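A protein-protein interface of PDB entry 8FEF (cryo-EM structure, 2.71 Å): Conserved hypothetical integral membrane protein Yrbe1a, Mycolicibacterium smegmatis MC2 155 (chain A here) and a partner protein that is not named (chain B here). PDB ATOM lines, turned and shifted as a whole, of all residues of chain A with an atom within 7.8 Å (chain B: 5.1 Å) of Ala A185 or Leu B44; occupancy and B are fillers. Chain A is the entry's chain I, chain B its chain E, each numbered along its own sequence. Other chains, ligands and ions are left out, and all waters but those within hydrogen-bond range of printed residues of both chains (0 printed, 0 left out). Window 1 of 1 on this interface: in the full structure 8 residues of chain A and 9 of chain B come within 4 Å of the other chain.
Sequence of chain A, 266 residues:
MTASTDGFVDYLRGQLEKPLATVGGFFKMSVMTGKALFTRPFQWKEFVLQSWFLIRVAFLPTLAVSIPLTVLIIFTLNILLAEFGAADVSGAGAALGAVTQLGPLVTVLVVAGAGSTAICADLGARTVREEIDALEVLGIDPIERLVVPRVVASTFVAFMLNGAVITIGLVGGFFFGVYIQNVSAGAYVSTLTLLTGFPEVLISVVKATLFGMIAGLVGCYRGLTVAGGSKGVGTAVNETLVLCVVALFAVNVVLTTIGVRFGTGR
Among the printed residues, pairs that only touch across the chains: Tyr A179 with Gly B46 (3.6 Å), Tyr A179 with Pro B45 (3.6 Å), Ala A185 with Leu B44 (3.7 Å), Gly A186 with Asn B70 (3.7 Å), Val A189 with Leu B44 (3.7 Å) and Phe A174 with Leu B44 (3.8 Å).
Of the 8 printed residues of chain B, 4 touch a printed residue of chain A. Printed residues of chain B that touch a printed residue of chain A: Leu B44, Pro B45, Gly B46 and Asn B70. Hydrophobic or aromatic side chains of chain B that line the printed part of chain A: Leu B44. Among the printed residues, no Asp or Glu carboxylate lies within 4 Å of a Lys or Arg side-chain nitrogen of the other chain.
The backbone NH (N) of Phe A174 is in hydrogen-bond range of the side-chain hydroxyl (OH) of Tyr A188 (3.5 Å). The backbone carbonyl oxygen (O) of Leu B44 lies within hydrogen-bond range of the guanidinium group (NH1) of Arg B82, at 2.8 Å. The backbone carbonyl oxygen (O) of Gly B46 sits close to the side-chain hydroxyl (OG1) of Thr B50 (3.3 Å). The side-chain amide nitrogen (ND2) of Asn B70 is in hydrogen-bond range of the backbone carbonyl oxygen (O) of Val B42, 2.5 Å away. O of Gly A186 lies within hydrogen-bond range of OG of Ser A190 (2.5 Å). The side-chain amide oxygen of Asn B70 lies within hydrogen-bond range of the backbone NH of Leu B44 (3.4 Å).
Of chain B, only Leu B44 comes within 4 Å of Ala A185. Leu B44 touches just these residues of chain A: Phe A174 (3.8 Å), Ala A185 (3.7 Å) and Val A189 (3.7 Å). Pro B45 touches one residue of chain A. Printed residues of chain B within 4 Å of Tyr A179: Pro B45 and Gly B46. Printed residues of chain B within 4 Å of Gly A186: Asn B70. The nearest residue of chain A that does not touch Leu B44 is Gly A186 (4.4 Å).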
ATOM      1  N   ASP A  88     -15.999  15.865   1.640  1.00  0.00           N
ATOM      2  CA  ASP A  88     -16.633  14.578   1.386  1.00  0.00           C
ATOM      3  C   ASP A  88     -15.860  13.713   0.403  1.00  0.00           C
ATOM      4  O   ASP A  88     -16.137  12.512   0.308  1.00  0.00           O
ATOM      5  CB  ASP A  88     -18.058  14.785   0.863  1.00  0.00           C
ATOM      6  CG  ASP A  88     -18.972  15.404   1.897  1.00  0.00           C
ATOM      7  OD1 ASP A  88     -18.740  15.182   3.104  1.00  0.00           O
ATOM      8  OD2 ASP A  88     -19.922  16.113   1.504  1.00  0.00           O
ATOM      9  N   PHE A 174      -9.574   5.926   7.954  1.00  0.00           N
ATOM     10  CA  PHE A 174     -11.008   5.972   8.229  1.00  0.00           C
ATOM     11  C   PHE A 174     -11.273   6.297   9.690  1.00  0.00           C
ATOM     12  O   PHE A 174     -12.036   7.219  10.006  1.00  0.00           O
ATOM     13  CB  PHE A 174     -11.660   4.638   7.863  1.00  0.00           C
ATOM     14  CG  PHE A 174     -13.042   4.461   8.432  1.00  0.00           C
ATOM     15  CD1 PHE A 174     -14.136   5.038   7.812  1.00  0.00           C
ATOM     16  CD2 PHE A 174     -13.250   3.703   9.573  1.00  0.00           C
ATOM     17  CE1 PHE A 174     -15.405   4.876   8.327  1.00  0.00           C
ATOM     18  CE2 PHE A 174     -14.519   3.541  10.093  1.00  0.00           C
ATOM     19  CZ  PHE A 174     -15.596   4.127   9.468  1.00  0.00           C
ATOM     20  N   GLY A 177     -10.103   9.952  10.677  1.00  0.00           N
ATOM     21  CA  GLY A 177     -10.946  10.988  10.107  1.00  0.00           C
ATOM     22  C   GLY A 177     -12.333  11.024  10.718  1.00  0.00           C
ATOM     23  O   GLY A 177     -12.896  12.099  10.939  1.00  0.00           O
ATOM     24  N   VAL A 178     -12.907   9.854  11.000  1.00  0.00           N
ATOM     25  CA  VAL A 178     -14.274   9.818  11.504  1.00  0.00           C
ATOM     26  C   VAL A 178     -14.322  10.181  12.984  1.00  0.00           C
ATOM     27  O   VAL A 178     -15.126  11.022  13.403  1.00  0.00           O
ATOM     28  CB  VAL A 178     -14.907   8.441  11.233  1.00  0.00           C
ATOM     29  CG1 VAL A 178     -16.224   8.305  11.973  1.00  0.00           C
ATOM     30  CG2 VAL A 178     -15.118   8.254   9.744  1.00  0.00           C
ATOM     31  N   TYR A 179     -13.462   9.569  13.799  1.00  0.00           N
ATOM     32  CA  TYR A 179     -13.541   9.721  15.245  1.00  0.00           C
ATOM     33  C   TYR A 179     -12.770  10.919  15.783  1.00  0.00           C
ATOM     34  O   TYR A 179     -12.881  11.210  16.979  1.00  0.00           O
ATOM     35  CB  TYR A 179     -13.035   8.449  15.936  1.00  0.00           C
ATOM     36  CG  TYR A 179     -14.012   7.294  15.919  1.00  0.00           C
ATOM     37  CD1 TYR A 179     -14.431   6.723  14.725  1.00  0.00           C
ATOM     38  CD2 TYR A 179     -14.508   6.766  17.103  1.00  0.00           C
ATOM     39  CE1 TYR A 179     -15.320   5.667  14.710  1.00  0.00           C
ATOM     40  CE2 TYR A 179     -15.397   5.709  17.099  1.00  0.00           C
ATOM     41  CZ  TYR A 179     -15.799   5.164  15.900  1.00  0.00           C
ATOM     42  OH  TYR A 179     -16.684   4.111  15.892  1.00  0.00           O
ATOM     43  N   ASN A 182     -14.119  14.364  12.596  1.00  0.00           N
ATOM     44  CA  ASN A 182     -15.575  14.430  12.457  1.00  0.00           C
ATOM     45  C   ASN A 182     -16.015  14.543  10.999  1.00  0.00           C
ATOM     46  O   ASN A 182     -16.941  15.288  10.671  1.00  0.00           O
ATOM     47  CB  ASN A 182     -16.153  15.581  13.283  1.00  0.00           C
ATOM     48  CG  ASN A 182     -15.966  15.379  14.771  1.00  0.00           C
ATOM     49  OD1 ASN A 182     -15.995  14.252  15.264  1.00  0.00           O
ATOM     50  ND2 ASN A 182     -15.771  16.474  15.496  1.00  0.00           N
ATOM     51  N   VAL A 183     -15.353  13.805  10.112  1.00  0.00           N
ATOM     52  CA  VAL A 183     -15.845  13.680   8.747  1.00  0.00           C
ATOM     53  C   VAL A 183     -16.902  12.585   8.728  1.00  0.00           C
ATOM     54  O   VAL A 183     -17.035  11.821   9.691  1.00  0.00           O
ATOM     55  CB  VAL A 183     -14.711  13.382   7.748  1.00  0.00           C
ATOM     56  CG1 VAL A 183     -13.574  14.374   7.923  1.00  0.00           C
ATOM     57  CG2 VAL A 183     -14.217  11.957   7.907  1.00  0.00           C
ATOM     58  N   SER A 184     -17.664  12.507   7.643  1.00  0.00           N
ATOM     59  CA  SER A 184     -18.711  11.503   7.521  1.00  0.00           C
ATOM     60  C   SER A 184     -18.113  10.185   7.038  1.00  0.00           C
ATOM     61  O   SER A 184     -17.342  10.154   6.074  1.00  0.00           O
ATOM     62  CB  SER A 184     -19.826  11.997   6.603  1.00  0.00           C
ATOM     63  OG  SER A 184     -19.368  12.200   5.293  1.00  0.00           O
ATOM     64  N   ALA A 185     -18.474   9.099   7.723  1.00  0.00           N
ATOM     65  CA  ALA A 185     -17.962   7.770   7.402  1.00  0.00           C
ATOM     66  C   ALA A 185     -18.430   7.277   6.037  1.00  0.00           C
ATOM     67  O   ALA A 185     -17.640   6.700   5.275  1.00  0.00           O
ATOM     68  CB  ALA A 185     -18.380   6.786   8.494  1.00  0.00           C
ATOM     69  N   GLY A 186     -19.711   7.475   5.717  1.00  0.00           N
ATOM     70  CA  GLY A 186     -20.205   7.078   4.411  1.00  0.00           C
ATOM     71  C   GLY A 186     -19.520   7.783   3.259  1.00  0.00           C
ATOM     72  O   GLY A 186     -19.324   7.189   2.199  1.00  0.00           O
ATOM     73  N   ALA A 187     -19.145   9.049   3.441  1.00  0.00           N
ATOM     74  CA  ALA A 187     -18.373   9.727   2.405  1.00  0.00           C
ATOM     75  C   ALA A 187     -16.985   9.132   2.256  1.00  0.00           C
ATOM     76  O   ALA A 187     -16.439   9.116   1.149  1.00  0.00           O
ATOM     77  CB  ALA A 187     -18.260  11.221   2.680  1.00  0.00           C
ATOM     78  N   TYR A 188     -16.390   8.662   3.351  1.00  0.00           N
ATOM     79  CA  TYR A 188     -15.077   8.044   3.243  1.00  0.00           C
ATOM     80  C   TYR A 188     -15.153   6.720   2.498  1.00  0.00           C
ATOM     81  O   TYR A 188     -14.376   6.481   1.567  1.00  0.00           O
ATOM     82  CB  TYR A 188     -14.477   7.839   4.634  1.00  0.00           C
ATOM     83  CG  TYR A 188     -13.051   7.341   4.612  1.00  0.00           C
ATOM     84  CD1 TYR A 188     -11.991   8.232   4.586  1.00  0.00           C
ATOM     85  CD2 TYR A 188     -12.764   5.982   4.597  1.00  0.00           C
ATOM     86  CE1 TYR A 188     -10.689   7.787   4.559  1.00  0.00           C
ATOM     87  CE2 TYR A 188     -11.463   5.529   4.558  1.00  0.00           C
ATOM     88  CZ  TYR A 188     -10.430   6.436   4.545  1.00  0.00           C
ATOM     89  OH  TYR A 188      -9.130   5.989   4.516  1.00  0.00           O
ATOM     90  N   VAL A 189     -16.090   5.847   2.876  1.00  0.00           N
ATOM     91  CA  VAL A 189     -16.070   4.521   2.262  1.00  0.00           C
ATOM     92  C   VAL A 189     -16.632   4.532   0.842  1.00  0.00           C
ATOM     93  O   VAL A 189     -16.268   3.680   0.025  1.00  0.00           O
ATOM     94  CB  VAL A 189     -16.814   3.508   3.144  1.00  0.00           C
ATOM     95  CG1 VAL A 189     -16.066   3.296   4.446  1.00  0.00           C
ATOM     96  CG2 VAL A 189     -18.234   3.973   3.404  1.00  0.00           C
ATOM     97  N   SER A 190     -17.515   5.476   0.517  1.00  0.00           N
ATOM     98  CA  SER A 190     -18.121   5.512  -0.809  1.00  0.00           C
ATOM     99  C   SER A 190     -17.285   6.244  -1.846  1.00  0.00           C
ATOM    100  O   SER A 190     -17.583   6.138  -3.040  1.00  0.00           O
ATOM    101  CB  SER A 190     -19.505   6.158  -0.746  1.00  0.00           C
ATOM    102  OG  SER A 190     -19.411   7.502  -0.318  1.00  0.00           O
ATOM    103  N   THR A 191     -16.261   6.983  -1.433  1.00  0.00           N
ATOM    104  CA  THR A 191     -15.424   7.720  -2.365  1.00  0.00           C
ATOM    105  C   THR A 191     -14.060   7.052  -2.560  1.00  0.00           C
ATOM    106  O   THR A 191     -13.260   7.511  -3.382  1.00  0.00           O
ATOM    107  CB  THR A 191     -15.315   9.173  -1.854  1.00  0.00           C
ATOM    108  OG1 THR A 191     -16.632   9.729  -1.798  1.00  0.00           O
ATOM    109  CG2 THR A 191     -14.582  10.074  -2.809  1.00  0.00           C
ATOM    110  N   LEU A 192     -13.807   5.928  -1.879  1.00  0.00           N
ATOM    111  CA  LEU A 192     -12.523   5.239  -2.008  1.00  0.00           C
ATOM    112  C   LEU A 192     -12.269   4.785  -3.441  1.00  0.00           C
ATOM    113  O   LEU A 192     -11.148   4.903  -3.948  1.00  0.00           O
ATOM    114  CB  LEU A 192     -12.462   4.037  -1.066  1.00  0.00           C
ATOM    115  CG  LEU A 192     -12.350   4.266   0.439  1.00  0.00           C
ATOM    116  CD1 LEU A 192     -12.376   2.941   1.175  1.00  0.00           C
ATOM    117  CD2 LEU A 192     -11.082   5.029   0.765  1.00  0.00           C
ATOM    118  N   VAL B  42     -21.691  -1.430   3.316  1.00  0.00           N
ATOM    119  CA  VAL B  42     -21.601  -2.209   4.549  1.00  0.00           C
ATOM    120  C   VAL B  42     -21.828  -1.274   5.732  1.00  0.00           C
ATOM    121  O   VAL B  42     -21.327  -0.140   5.729  1.00  0.00           O
ATOM    122  CB  VAL B  42     -20.255  -2.957   4.631  1.00  0.00           C
ATOM    123  CG1 VAL B  42     -19.078  -1.994   4.676  1.00  0.00           C
ATOM    124  CG2 VAL B  42     -20.221  -3.891   5.830  1.00  0.00           C
ATOM    125  N   PRO B  43     -22.639  -1.663   6.718  1.00  0.00           N
ATOM    126  CA  PRO B  43     -22.849  -0.796   7.885  1.00  0.00           C
ATOM    127  C   PRO B  43     -21.547  -0.532   8.627  1.00  0.00           C
ATOM    128  O   PRO B  43     -20.702  -1.416   8.773  1.00  0.00           O
ATOM    129  CB  PRO B  43     -23.839  -1.591   8.744  1.00  0.00           C
ATOM    130  CG  PRO B  43     -24.525  -2.496   7.787  1.00  0.00           C
ATOM    131  CD  PRO B  43     -23.498  -2.859   6.762  1.00  0.00           C
ATOM    132  N   LEU B  44     -21.395   0.701   9.101  1.00  0.00           N
ATOM    133  CA  LEU B  44     -20.181   1.119   9.774  1.00  0.00           C
ATOM    134  C   LEU B  44     -20.465   1.450  11.233  1.00  0.00           C
ATOM    135  O   LEU B  44     -21.543   1.952  11.561  1.00  0.00           O
ATOM    136  CB  LEU B  44     -19.565   2.342   9.084  1.00  0.00           C
ATOM    137  CG  LEU B  44     -19.169   2.138   7.623  1.00  0.00           C
ATOM    138  CD1 LEU B  44     -18.672   3.438   7.031  1.00  0.00           C
ATOM    139  CD2 LEU B  44     -18.113   1.055   7.502  1.00  0.00           C
ATOM    140  N   PRO B  45     -19.523   1.174  12.131  1.00  0.00           N
ATOM    141  CA  PRO B  45     -19.746   1.472  13.548  1.00  0.00           C
ATOM    142  C   PRO B  45     -19.638   2.961  13.836  1.00  0.00           C
ATOM    143  O   PRO B  45     -19.003   3.725  13.107  1.00  0.00           O
ATOM    144  CB  PRO B  45     -18.633   0.689  14.250  1.00  0.00           C
ATOM    145  CG  PRO B  45     -17.541   0.636  13.242  1.00  0.00           C
ATOM    146  CD  PRO B  45     -18.218   0.529  11.902  1.00  0.00           C
ATOM    147  N   GLY B  46     -20.281   3.365  14.927  1.00  0.00           N
ATOM    148  CA  GLY B  46     -20.193   4.728  15.404  1.00  0.00           C
ATOM    149  C   GLY B  46     -21.153   5.668  14.698  1.00  0.00           C
ATOM    150  O   GLY B  46     -21.785   5.339  13.694  1.00  0.00           O
ATOM    151  N   THR B  50     -26.375   4.684  16.041  1.00  0.00           N
ATOM    152  CA  THR B  50     -25.726   3.436  16.414  1.00  0.00           C
ATOM    153  C   THR B  50     -25.658   3.227  17.920  1.00  0.00           C
ATOM    154  O   THR B  50     -25.345   2.117  18.360  1.00  0.00           O
ATOM    155  CB  THR B  50     -24.311   3.380  15.832  1.00  0.00           C
ATOM    156  OG1 THR B  50     -23.546   4.484  16.328  1.00  0.00           O
ATOM    157  CG2 THR B  50     -24.363   3.448  14.316  1.00  0.00           C
ATOM    158  N   ASN B  70     -25.057   3.901   4.660  1.00  0.00           N
ATOM    159  CA  ASN B  70     -24.293   4.748   5.578  1.00  0.00           C
ATOM    160  C   ASN B  70     -24.439   6.231   5.253  1.00  0.00           C
ATOM    161  O   ASN B  70     -23.638   7.050   5.709  1.00  0.00           O
ATOM    162  CB  ASN B  70     -22.808   4.361   5.619  1.00  0.00           C
ATOM    163  CG  ASN B  70     -22.599   2.893   5.911  1.00  0.00           C
ATOM    164  OD1 ASN B  70     -23.290   2.311   6.745  1.00  0.00           O
ATOM    165  ND2 ASN B  70     -21.648   2.283   5.217  1.00  0.00           N
ATOM    166  N   ARG B  82     -28.624   7.419  10.418  1.00  0.00           N
ATOM    167  CA  ARG B  82     -27.902   6.731   9.359  1.00  0.00           C
ATOM    168  C   ARG B  82     -28.819   5.708   8.704  1.00  0.00           C
ATOM    169  O   ARG B  82     -29.649   5.093   9.377  1.00  0.00           O
ATOM    170  CB  ARG B  82     -26.651   6.037   9.920  1.00  0.00           C
ATOM    171  CG  ARG B  82     -25.838   5.259   8.906  1.00  0.00           C
ATOM    172  CD  ARG B  82     -25.050   4.150   9.575  1.00  0.00           C
ATOM    173  NE  ARG B  82     -25.918   3.259  10.334  1.00  0.00           N
ATOM    174  CZ  ARG B  82     -25.509   2.158  10.948  1.00  0.00           C
ATOM    175  NH1 ARG B  82     -24.244   1.775  10.908  1.00  0.00           N
ATOM    176  NH2 ARG B  82     -26.391   1.423  11.618  1.00  0.00           N
